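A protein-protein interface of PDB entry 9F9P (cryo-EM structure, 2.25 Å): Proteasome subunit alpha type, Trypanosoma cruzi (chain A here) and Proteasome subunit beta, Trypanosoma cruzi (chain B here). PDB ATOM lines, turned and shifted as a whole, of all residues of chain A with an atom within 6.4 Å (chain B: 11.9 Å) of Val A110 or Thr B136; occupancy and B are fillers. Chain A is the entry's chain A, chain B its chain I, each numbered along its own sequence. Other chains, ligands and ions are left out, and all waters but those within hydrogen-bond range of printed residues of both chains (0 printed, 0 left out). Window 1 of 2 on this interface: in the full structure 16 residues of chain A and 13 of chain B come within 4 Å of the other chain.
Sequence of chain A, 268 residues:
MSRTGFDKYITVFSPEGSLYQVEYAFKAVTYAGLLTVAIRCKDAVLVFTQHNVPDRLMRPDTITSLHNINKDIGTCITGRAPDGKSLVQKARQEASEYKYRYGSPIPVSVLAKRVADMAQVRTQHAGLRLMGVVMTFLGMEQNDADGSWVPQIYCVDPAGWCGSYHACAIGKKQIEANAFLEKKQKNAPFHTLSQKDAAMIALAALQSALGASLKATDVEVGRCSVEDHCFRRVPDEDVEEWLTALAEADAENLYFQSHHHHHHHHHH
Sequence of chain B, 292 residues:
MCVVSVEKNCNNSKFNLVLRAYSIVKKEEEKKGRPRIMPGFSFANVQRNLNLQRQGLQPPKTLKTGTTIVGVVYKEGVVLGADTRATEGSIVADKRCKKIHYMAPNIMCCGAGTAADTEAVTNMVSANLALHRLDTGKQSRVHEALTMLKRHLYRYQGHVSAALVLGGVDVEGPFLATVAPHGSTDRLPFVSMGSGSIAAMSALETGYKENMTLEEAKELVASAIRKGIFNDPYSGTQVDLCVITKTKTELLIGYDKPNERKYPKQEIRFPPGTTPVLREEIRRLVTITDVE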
ATOM      1  N   TYR A  98      33.803 -11.233   1.870  1.00  0.00           N
ATOM      2  CA  TYR A  98      33.006 -11.352   3.065  1.00  0.00           C
ATOM      3  C   TYR A  98      32.766  -9.976   3.703  1.00  0.00           C
ATOM      4  O   TYR A  98      31.665  -9.668   4.095  1.00  0.00           O
ATOM      5  CB  TYR A  98      33.663 -12.365   4.019  1.00  0.00           C
ATOM      6  CG  TYR A  98      32.921 -12.632   5.294  1.00  0.00           C
ATOM      7  CD1 TYR A  98      32.218 -13.814   5.494  1.00  0.00           C
ATOM      8  CD2 TYR A  98      33.001 -11.743   6.354  1.00  0.00           C
ATOM      9  CE1 TYR A  98      31.562 -14.088   6.697  1.00  0.00           C
ATOM     10  CE2 TYR A  98      32.339 -11.986   7.563  1.00  0.00           C
ATOM     11  CZ  TYR A  98      31.582 -13.141   7.715  1.00  0.00           C
ATOM     12  OH  TYR A  98      30.945 -13.325   8.939  1.00  0.00           O
ATOM     13  N   ILE A 106      36.184 -11.319   8.373  1.00  0.00           N
ATOM     14  CA  ILE A 106      35.794 -12.726   8.403  1.00  0.00           C
ATOM     15  C   ILE A 106      36.394 -13.407   9.619  1.00  0.00           C
ATOM     16  O   ILE A 106      37.564 -13.272   9.875  1.00  0.00           O
ATOM     17  CB  ILE A 106      36.234 -13.420   7.092  1.00  0.00           C
ATOM     18  CG1 ILE A 106      35.616 -14.808   6.934  1.00  0.00           C
ATOM     19  CG2 ILE A 106      37.751 -13.466   6.945  1.00  0.00           C
ATOM     20  CD1 ILE A 106      35.705 -15.331   5.512  1.00  0.00           C
ATOM     21  N   PRO A 107      35.638 -14.167  10.408  1.00  0.00           N
ATOM     22  CA  PRO A 107      36.218 -15.003  11.461  1.00  0.00           C
ATOM     23  C   PRO A 107      37.096 -16.165  10.968  1.00  0.00           C
ATOM     24  O   PRO A 107      36.791 -16.782   9.966  1.00  0.00           O
ATOM     25  CB  PRO A 107      35.000 -15.630  12.144  1.00  0.00           C
ATOM     26  CG  PRO A 107      33.866 -14.737  11.769  1.00  0.00           C
ATOM     27  CD  PRO A 107      34.169 -14.254  10.361  1.00  0.00           C
ATOM     28  N   VAL A 108      38.149 -16.507  11.710  1.00  0.00           N
ATOM     29  CA  VAL A 108      39.107 -17.482  11.239  1.00  0.00           C
ATOM     30  C   VAL A 108      38.500 -18.875  11.030  1.00  0.00           C
ATOM     31  O   VAL A 108      38.834 -19.530  10.064  1.00  0.00           O
ATOM     32  CB  VAL A 108      40.364 -17.516  12.107  1.00  0.00           C
ATOM     33  CG1 VAL A 108      40.055 -17.871  13.525  1.00  0.00           C
ATOM     34  CG2 VAL A 108      41.384 -18.485  11.542  1.00  0.00           C
ATOM     35  N   SER A 109      37.504 -19.284  11.800  1.00  0.00           N
ATOM     36  CA  SER A 109      36.853 -20.567  11.566  1.00  0.00           C
ATOM     37  C   SER A 109      36.028 -20.575  10.278  1.00  0.00           C
ATOM     38  O   SER A 109      35.828 -21.626   9.713  1.00  0.00           O
ATOM     39  CB  SER A 109      35.932 -20.904  12.709  1.00  0.00           C
ATOM     40  OG  SER A 109      35.050 -19.796  12.930  1.00  0.00           O
ATOM     41  N   VAL A 110      35.431 -19.441   9.905  1.00  0.00           N
ATOM     42  CA  VAL A 110      34.633 -19.349   8.701  1.00  0.00           C
ATOM     43  C   VAL A 110      35.516 -19.367   7.468  1.00  0.00           C
ATOM     44  O   VAL A 110      35.157 -19.980   6.484  1.00  0.00           O
ATOM     45  CB  VAL A 110      33.721 -18.094   8.707  1.00  0.00           C
ATOM     46  CG1 VAL A 110      32.974 -17.899   7.392  1.00  0.00           C
ATOM     47  CG2 VAL A 110      32.697 -18.204   9.811  1.00  0.00           C
ATOM     48  N   LEU A 111      36.615 -18.643   7.496  1.00  0.00           N
ATOM     49  CA  LEU A 111      37.560 -18.613   6.390  1.00  0.00           C
ATOM     50  C   LEU A 111      38.138 -19.992   6.108  1.00  0.00           C
ATOM     51  O   LEU A 111      38.272 -20.363   4.952  1.00  0.00           O
ATOM     52  CB  LEU A 111      38.707 -17.663   6.734  1.00  0.00           C
ATOM     53  CG  LEU A 111      39.831 -17.648   5.691  1.00  0.00           C
ATOM     54  CD1 LEU A 111      39.502 -16.783   4.497  1.00  0.00           C
ATOM     55  CD2 LEU A 111      41.099 -17.199   6.320  1.00  0.00           C
ATOM     56  N   ALA A 112      38.544 -20.717   7.137  1.00  0.00           N
ATOM     57  CA  ALA A 112      39.095 -22.051   6.966  1.00  0.00           C
ATOM     58  C   ALA A 112      38.121 -22.988   6.273  1.00  0.00           C
ATOM     59  O   ALA A 112      38.507 -23.740   5.402  1.00  0.00           O
ATOM     60  CB  ALA A 112      39.483 -22.633   8.311  1.00  0.00           C
ATOM     61  N   LYS A 113      36.862 -22.931   6.643  1.00  0.00           N
ATOM     62  CA  LYS A 113      35.818 -23.694   5.979  1.00  0.00           C
ATOM     63  C   LYS A 113      35.628 -23.311   4.506  1.00  0.00           C
ATOM     64  O   LYS A 113      35.380 -24.169   3.674  1.00  0.00           O
ATOM     65  CB  LYS A 113      34.531 -23.468   6.750  1.00  0.00           C
ATOM     66  CG  LYS A 113      33.535 -24.603   6.672  1.00  0.00           C
ATOM     67  CD  LYS A 113      32.336 -24.413   7.605  1.00  0.00           C
ATOM     68  CE  LYS A 113      31.093 -25.162   7.142  1.00  0.00           C
ATOM     69  NZ  LYS A 113      29.860 -24.753   7.871  1.00  0.00           N
ATOM     70  N   ARG A 114      35.744 -22.036   4.154  1.00  0.00           N
ATOM     71  CA  ARG A 114      35.619 -21.635   2.767  1.00  0.00           C
ATOM     72  C   ARG A 114      36.757 -22.142   1.889  1.00  0.00           C
ATOM     73  O   ARG A 114      36.532 -22.415   0.722  1.00  0.00           O
ATOM     74  CB  ARG A 114      35.657 -20.121   2.606  1.00  0.00           C
ATOM     75  CG  ARG A 114      34.510 -19.410   3.285  1.00  0.00           C
ATOM     76  CD  ARG A 114      33.186 -19.680   2.608  1.00  0.00           C
ATOM     77  NE  ARG A 114      32.454 -18.423   2.762  1.00  0.00           N
ATOM     78  CZ  ARG A 114      31.446 -18.238   3.615  1.00  0.00           C
ATOM     79  NH1 ARG A 114      30.815 -17.075   3.652  1.00  0.00           N
ATOM     80  NH2 ARG A 114      31.061 -19.245   4.393  1.00  0.00           N
ATOM     81  N   VAL A 115      37.973 -22.153   2.416  1.00  0.00           N
ATOM     82  CA  VAL A 115      39.119 -22.699   1.718  1.00  0.00           C
ATOM     83  C   VAL A 115      39.029 -24.214   1.659  1.00  0.00           C
ATOM     84  O   VAL A 115      39.440 -24.810   0.688  1.00  0.00           O
ATOM     85  CB  VAL A 115      40.413 -22.252   2.428  1.00  0.00           C
ATOM     86  CG1 VAL A 115      41.649 -22.932   1.908  1.00  0.00           C
ATOM     87  CG2 VAL A 115      40.602 -20.750   2.337  1.00  0.00           C
ATOM     88  N   GLU A 141      39.380 -15.288  18.039  1.00  0.00           N
ATOM     89  CA  GLU A 141      37.937 -15.284  17.803  1.00  0.00           C
ATOM     90  C   GLU A 141      37.166 -14.904  19.075  1.00  0.00           C
ATOM     91  O   GLU A 141      37.526 -15.303  20.191  1.00  0.00           O
ATOM     92  CB  GLU A 141      37.534 -16.695  17.385  1.00  0.00           C
ATOM     93  CG  GLU A 141      36.340 -16.783  16.449  1.00  0.00           C
ATOM     94  CD  GLU A 141      36.379 -17.932  15.436  1.00  0.00           C
ATOM     95  OE1 GLU A 141      35.697 -18.960  15.660  1.00  0.00           O
ATOM     96  OE2 GLU A 141      37.031 -17.781  14.392  1.00  0.00           O
ATOM     97  N   ALA B 104      15.674 -11.540  13.459  1.00  0.00           N
ATOM     98  CA  ALA B 104      16.462 -12.558  14.119  1.00  0.00           C
ATOM     99  C   ALA B 104      16.035 -12.648  15.571  1.00  0.00           C
ATOM    100  O   ALA B 104      15.284 -11.832  16.041  1.00  0.00           O
ATOM    101  CB  ALA B 104      17.928 -12.197  13.980  1.00  0.00           C
ATOM    102  N   PRO B 105      16.435 -13.639  16.362  1.00  0.00           N
ATOM    103  CA  PRO B 105      16.070 -13.632  17.786  1.00  0.00           C
ATOM    104  C   PRO B 105      16.448 -12.370  18.592  1.00  0.00           C
ATOM    105  O   PRO B 105      15.765 -11.998  19.535  1.00  0.00           O
ATOM    106  CB  PRO B 105      16.859 -14.840  18.347  1.00  0.00           C
ATOM    107  CG  PRO B 105      17.017 -15.789  17.149  1.00  0.00           C
ATOM    108  CD  PRO B 105      17.178 -14.849  15.945  1.00  0.00           C
ATOM    109  N   ASN B 106      17.513 -11.680  18.187  1.00  0.00           N
ATOM    110  CA  ASN B 106      17.954 -10.472  18.853  1.00  0.00           C
ATOM    111  C   ASN B 106      17.782  -9.218  17.999  1.00  0.00           C
ATOM    112  O   ASN B 106      18.396  -8.234  18.327  1.00  0.00           O
ATOM    113  CB  ASN B 106      19.427 -10.664  19.268  1.00  0.00           C
ATOM    114  CG  ASN B 106      20.352 -10.912  18.103  1.00  0.00           C
ATOM    115  OD1 ASN B 106      20.052 -11.620  17.151  1.00  0.00           O
ATOM    116  ND2 ASN B 106      21.484 -10.251  18.140  1.00  0.00           N
ATOM    117  N   ALA B 127      16.022 -14.320   5.990  1.00  0.00           N
ATOM    118  CA  ALA B 127      16.438 -15.631   5.532  1.00  0.00           C
ATOM    119  C   ALA B 127      17.952 -15.766   5.351  1.00  0.00           C
ATOM    120  O   ALA B 127      18.475 -16.816   5.666  1.00  0.00           O
ATOM    121  CB  ALA B 127      15.758 -15.931   4.227  1.00  0.00           C
ATOM    122  N   ASN B 128      18.628 -14.777   4.760  1.00  0.00           N
ATOM    123  CA  ASN B 128      20.085 -14.789   4.651  1.00  0.00           C
ATOM    124  C   ASN B 128      20.808 -14.696   5.997  1.00  0.00           C
ATOM    125  O   ASN B 128      21.852 -15.310   6.139  1.00  0.00           O
ATOM    126  CB  ASN B 128      20.586 -13.719   3.689  1.00  0.00           C
ATOM    127  CG  ASN B 128      20.254 -14.074   2.246  1.00  0.00           C
ATOM    128  OD1 ASN B 128      20.296 -15.247   1.850  1.00  0.00           O
ATOM    129  ND2 ASN B 128      19.924 -13.085   1.433  1.00  0.00           N
ATOM    130  N   LEU B 129      20.254 -14.021   7.002  1.00  0.00           N
ATOM    131  CA  LEU B 129      20.837 -14.075   8.339  1.00  0.00           C
ATOM    132  C   LEU B 129      20.700 -15.446   8.973  1.00  0.00           C
ATOM    133  O   LEU B 129      21.547 -15.776   9.783  1.00  0.00           O
ATOM    134  CB  LEU B 129      20.220 -13.064   9.320  1.00  0.00           C
ATOM    135  CG  LEU B 129      20.522 -11.589   9.104  1.00  0.00           C
ATOM    136  CD1 LEU B 129      19.602 -10.783   9.971  1.00  0.00           C
ATOM    137  CD2 LEU B 129      21.945 -11.185   9.413  1.00  0.00           C
ATOM    138  N   ALA B 130      19.623 -16.176   8.692  1.00  0.00           N
ATOM    139  CA  ALA B 130      19.403 -17.507   9.273  1.00  0.00           C
ATOM    140  C   ALA B 130      20.381 -18.541   8.704  1.00  0.00           C
ATOM    141  O   ALA B 130      20.929 -19.331   9.457  1.00  0.00           O
ATOM    142  CB  ALA B 130      17.964 -17.966   9.114  1.00  0.00           C
ATOM    143  N   LEU B 131      20.624 -18.490   7.407  1.00  0.00           N
ATOM    144  CA  LEU B 131      21.672 -19.279   6.762  1.00  0.00           C
ATOM    145  C   LEU B 131      23.057 -19.010   7.357  1.00  0.00           C
ATOM    146  O   LEU B 131      23.869 -19.889   7.558  1.00  0.00           O
ATOM    147  CB  LEU B 131      21.755 -18.901   5.283  1.00  0.00           C
ATOM    148  CG  LEU B 131      21.169 -19.820   4.211  1.00  0.00           C
ATOM    149  CD1 LEU B 131      20.374 -21.026   4.715  1.00  0.00           C
ATOM    150  CD2 LEU B 131      20.349 -19.019   3.207  1.00  0.00           C
ATOM    151  N   HIS B 132      23.354 -17.758   7.615  1.00  0.00           N
ATOM    152  CA  HIS B 132      24.648 -17.379   8.131  1.00  0.00           C
ATOM    153  C   HIS B 132      24.827 -17.816   9.577  1.00  0.00           C
ATOM    154  O   HIS B 132      25.934 -18.169   9.921  1.00  0.00           O
ATOM    155  CB  HIS B 132      24.787 -15.886   7.899  1.00  0.00           C
ATOM    156  CG  HIS B 132      26.141 -15.330   8.152  1.00  0.00           C
ATOM    157  ND1 HIS B 132      26.309 -14.307   9.060  1.00  0.00           N
ATOM    158  CD2 HIS B 132      27.354 -15.578   7.595  1.00  0.00           C
ATOM    159  CE1 HIS B 132      27.581 -13.959   9.041  1.00  0.00           C
ATOM    160  NE2 HIS B 132      28.237 -14.741   8.202  1.00  0.00           N
ATOM    161  N   ARG B 133      23.774 -17.846  10.406  1.00  0.00           N
ATOM    162  CA  ARG B 133      23.899 -18.404  11.739  1.00  0.00           C
ATOM    163  C   ARG B 133      24.171 -19.910  11.742  1.00  0.00           C
ATOM    164  O   ARG B 133      24.717 -20.406  12.711  1.00  0.00           O
ATOM    165  CB  ARG B 133      22.620 -18.314  12.582  1.00  0.00           C
ATOM    166  CG  ARG B 133      22.318 -16.946  13.150  1.00  0.00           C
ATOM    167  CD  ARG B 133      21.332 -16.881  14.319  1.00  0.00           C
ATOM    168  NE  ARG B 133      19.975 -17.234  13.940  1.00  0.00           N
ATOM    169  CZ  ARG B 133      19.203 -16.545  13.114  1.00  0.00           C
ATOM    170  NH1 ARG B 133      19.545 -15.357  12.660  1.00  0.00           N
ATOM    171  NH2 ARG B 133      18.064 -17.066  12.714  1.00  0.00           N
ATOM    172  N   LEU B 134      23.616 -20.677  10.784  1.00  0.00           N
ATOM    173  CA  LEU B 134      23.824 -22.125  10.720  1.00  0.00           C
ATOM    174  C   LEU B 134      25.239 -22.431  10.259  1.00  0.00           C
ATOM    175  O   LEU B 134      25.882 -23.292  10.824  1.00  0.00           O
ATOM    176  CB  LEU B 134      22.827 -22.781   9.766  1.00  0.00           C
ATOM    177  CG  LEU B 134      21.399 -22.805  10.294  1.00  0.00           C
ATOM    178  CD1 LEU B 134      20.438 -23.421   9.305  1.00  0.00           C
ATOM    179  CD2 LEU B 134      21.323 -23.502  11.635  1.00  0.00           C
ATOM    180  N   ASP B 135      25.725 -21.682   9.284  1.00  0.00           N
ATOM    181  CA  ASP B 135      27.076 -21.813   8.765  1.00  0.00           C
ATOM    182  C   ASP B 135      28.075 -21.507   9.887  1.00  0.00           C
ATOM    183  O   ASP B 135      28.747 -22.408  10.385  1.00  0.00           O
ATOM    184  CB  ASP B 135      27.159 -20.934   7.514  1.00  0.00           C
ATOM    185  CG  ASP B 135      28.409 -21.006   6.653  1.00  0.00           C
ATOM    186  OD1 ASP B 135      29.062 -19.939   6.490  1.00  0.00           O
ATOM    187  OD2 ASP B 135      28.686 -22.108   6.086  1.00  0.00           O
ATOM    188  N   THR B 136      28.121 -20.255  10.355  1.00  0.00           N
ATOM    189  CA  THR B 136      29.081 -19.811  11.361  1.00  0.00           C
ATOM    190  C   THR B 136      28.863 -20.348  12.777  1.00  0.00           C
ATOM    191  O   THR B 136      29.793 -20.340  13.562  1.00  0.00           O
ATOM    192  CB  THR B 136      29.018 -18.292  11.552  1.00  0.00           C
ATOM    193  OG1 THR B 136      27.757 -17.894  12.113  1.00  0.00           O
ATOM    194  CG2 THR B 136      29.237 -17.556  10.255  1.00  0.00           C
ATOM    195  N   GLY B 137      27.646 -20.644  13.195  1.00  0.00           N
ATOM    196  CA  GLY B 137      27.438 -21.036  14.578  1.00  0.00           C
ATOM    197  C   GLY B 137      27.329 -19.876  15.578  1.00  0.00           C
ATOM    198  O   GLY B 137      27.312 -20.118  16.779  1.00  0.00           O
ATOM    199  N   LYS B 138      27.224 -18.619  15.122  1.00  0.00           N
ATOM    200  CA  LYS B 138      27.224 -17.471  16.029  1.00  0.00           C
ATOM    201  C   LYS B 138      25.986 -16.587  15.866  1.00  0.00           C
ATOM    202  O   LYS B 138      25.413 -16.503  14.784  1.00  0.00           O
ATOM    203  CB  LYS B 138      28.442 -16.595  15.755  1.00  0.00           C
ATOM    204  CG  LYS B 138      29.786 -17.269  16.001  1.00  0.00           C
ATOM    205  CD  LYS B 138      30.863 -16.732  15.096  1.00  0.00           C
ATOM    206  CE  LYS B 138      32.056 -17.664  14.980  1.00  0.00           C
ATOM    207  NZ  LYS B 138      33.298 -16.917  14.651  1.00  0.00           N
ATOM    208  N   GLN B 139      25.644 -15.880  16.946  1.00  0.00           N
ATOM    209  CA  GLN B 139      24.552 -14.914  17.004  1.00  0.00           C
ATOM    210  C   GLN B 139      24.692 -13.833  15.931  1.00  0.00           C
ATOM    211  O   GLN B 139      25.794 -13.355  15.654  1.00  0.00           O
ATOM    212  CB  GLN B 139      24.578 -14.282  18.400  1.00  0.00           C
ATOM    213  CG  GLN B 139      23.409 -13.351  18.693  1.00  0.00           C
ATOM    214  CD  GLN B 139      23.493 -12.629  20.017  1.00  0.00           C
ATOM    215  OE1 GLN B 139      24.445 -11.907  20.314  1.00  0.00           O
ATOM    216  NE2 GLN B 139      22.424 -12.748  20.780  1.00  0.00           N
ATOM    217  N   SER B 140      23.573 -13.409  15.343  1.00  0.00           N
ATOM    218  CA  SER B 140      23.611 -12.379  14.308  1.00  0.00           C
ATOM    219  C   SER B 140      23.941 -11.018  14.916  1.00  0.00           C
ATOM    220  O   SER B 140      23.538 -10.703  16.037  1.00  0.00           O
ATOM    221  CB  SER B 140      22.334 -12.339  13.509  1.00  0.00           C
ATOM    222  OG  SER B 140      21.930 -13.628  12.990  1.00  0.00           O
ATOM    223  N   ARG B 141      24.743 -10.237  14.195  1.00  0.00           N
ATOM    224  CA  ARG B 141      25.138  -8.901  14.596  1.00  0.00           C
ATOM    225  C   ARG B 141      24.233  -7.889  13.891  1.00  0.00           C
ATOM    226  O   ARG B 141      23.898  -8.057  12.713  1.00  0.00           O
ATOM    227  CB  ARG B 141      26.575  -8.567  14.170  1.00  0.00           C
ATOM    228  CG  ARG B 141      27.699  -9.487  14.642  1.00  0.00           C
ATOM    229  CD  ARG B 141      27.901  -9.402  16.140  1.00  0.00           C
ATOM    230  NE  ARG B 141      29.061 -10.168  16.616  1.00  0.00           N
ATOM    231  CZ  ARG B 141      30.255  -9.671  16.968  1.00  0.00           C
ATOM    232  NH1 ARG B 141      31.185 -10.483  17.437  1.00  0.00           N
ATOM    233  NH2 ARG B 141      30.529  -8.383  16.868  1.00  0.00           N
ATOM    234  N   GLU B 144      25.507  -6.357  10.664  1.00  0.00           N
ATOM    235  CA  GLU B 144      25.450  -7.185   9.457  1.00  0.00           C
ATOM    236  C   GLU B 144      24.113  -7.007   8.762  1.00  0.00           C
ATOM    237  O   GLU B 144      24.047  -6.908   7.558  1.00  0.00           O
ATOM    238  CB  GLU B 144      25.666  -8.693   9.711  1.00  0.00           C
ATOM    239  CG  GLU B 144      27.029  -9.031  10.354  1.00  0.00           C
ATOM    240  CD  GLU B 144      27.312 -10.481  10.848  1.00  0.00           C
ATOM    241  OE1 GLU B 144      26.444 -11.109  11.574  1.00  0.00           O
ATOM    242  OE2 GLU B 144      28.445 -11.002  10.535  1.00  0.00           O
ATOM    243  N   MET B 148      23.573  -5.599   4.897  1.00  0.00           N
ATOM    244  CA  MET B 148      22.809  -6.318   3.892  1.00  0.00           C
ATOM    245  C   MET B 148      21.588  -5.538   3.364  1.00  0.00           C
ATOM    246  O   MET B 148      21.313  -5.600   2.165  1.00  0.00           O
ATOM    247  CB  MET B 148      22.347  -7.654   4.481  1.00  0.00           C
ATOM    248  CG  MET B 148      23.498  -8.628   4.781  1.00  0.00           C
ATOM    249  SD  MET B 148      23.104  -9.823   6.160  1.00  0.00           S
ATOM    250  CE  MET B 148      22.370 -11.098   5.148  1.00  0.00           C
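Of the printed residues of chain B, Tyr A98 touches His B132 and Glu B144.
Ile A106 touches none of the printed residues of chain B.
Pro A107 touches just one residue of chain B: Lys B138 (3.3 Å).
Val A108 touches none of the printed residues of chain B.
Ser A109 touches one residue of chain B.
Printed residues of chain B within 4 Å of Val A110: Thr B136.
No residue of chain B comes within 4 Å of Leu A111.
No residue of chain B comes within 4 Å of Ala A112.
Lys A113 touches one residue of chain B.
Of the printed residues of chain B, Arg A114 touches Asp B135.
Val A115 touches none of the printed residues of chain B.
Of the printed residues of chain B, Glu A141 touches Lys B138.
Asn B128 touches none of the printed residues of chain A.
Printed residues of chain A within 4 Å of Asp B135: Lys A113 and Arg A114.
Thr B136 touches just one residue of chain A: Val A110.
Printed residues of chain A within 4 Å of Glu B144: Tyr A98 (3.8 Å).
The nearest residue of chain B that does not touch Val A110 is Asp B135 (4.5 Å).
The nearest residue of chain A that does not touch Thr B136 is Tyr A98 (4.7 Å).
The nearest printed residue of chain A that does not touch His B132 is Arg A114 (5.5 Å).
The side-chain amino group of Lys B138 is in salt-bridge range of the side-chain carboxylate of Glu A141 (3.3 Å).
A ring nitrogen (NE2) of His B132 lies within hydrogen-bond range of the side-chain hydroxyl of Tyr A98, at 3.1 Å.
NZ of Lys A113 lies within salt-bridge range of OD2 of Asp B135 (3.4 Å).
OD1 of Asp B135 is in salt-bridge range of NH2 of Arg A114 (3.0 Å).
The backbone NH of Val A108 lies close to the side-chain carboxylate of Glu A141, at 3.2 Å.
OE1 of Glu A141 is in hydrogen-bond range of OG of Ser A109 (2.9 Å).
The backbone NH (N) of Arg B141 sits at hydrogen-bond distance from the side-chain carboxylate (OE1) of Glu B144 (3.2 Å).
O of His B132 sits at hydrogen-bond distance from OG1 of Thr B136, 2.9 Å away.
The backbone NH (N) of Lys B138 lies within hydrogen-bond range of the side-chain hydroxyl (OG1) of Thr B136, 3.1 Å away.
Of the 12 printed residues of chain A, 7 touch a printed residue of chain B.
Hydrophobic or aromatic side chains of chain B that line the printed part of chain A: His B132.
Among the printed residues, Asp or Glu carboxylates within 4 Å of a Lys or Arg side-chain nitrogen of the other chain: Lys A113 with Asp B135 (3.4 Å), Arg A114 with Asp B135 (3.0 Å) and Glu A141 with Lys B138 (3.3 Å).
Glu B144 touches Tyr A98.
Pro A107 touches Lys B138 (CB to NZ, 3.3 Å).
OG of Ser A109 touches NZ of Lys B138 (3.8 Å).
Val A110 touches Thr B136.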
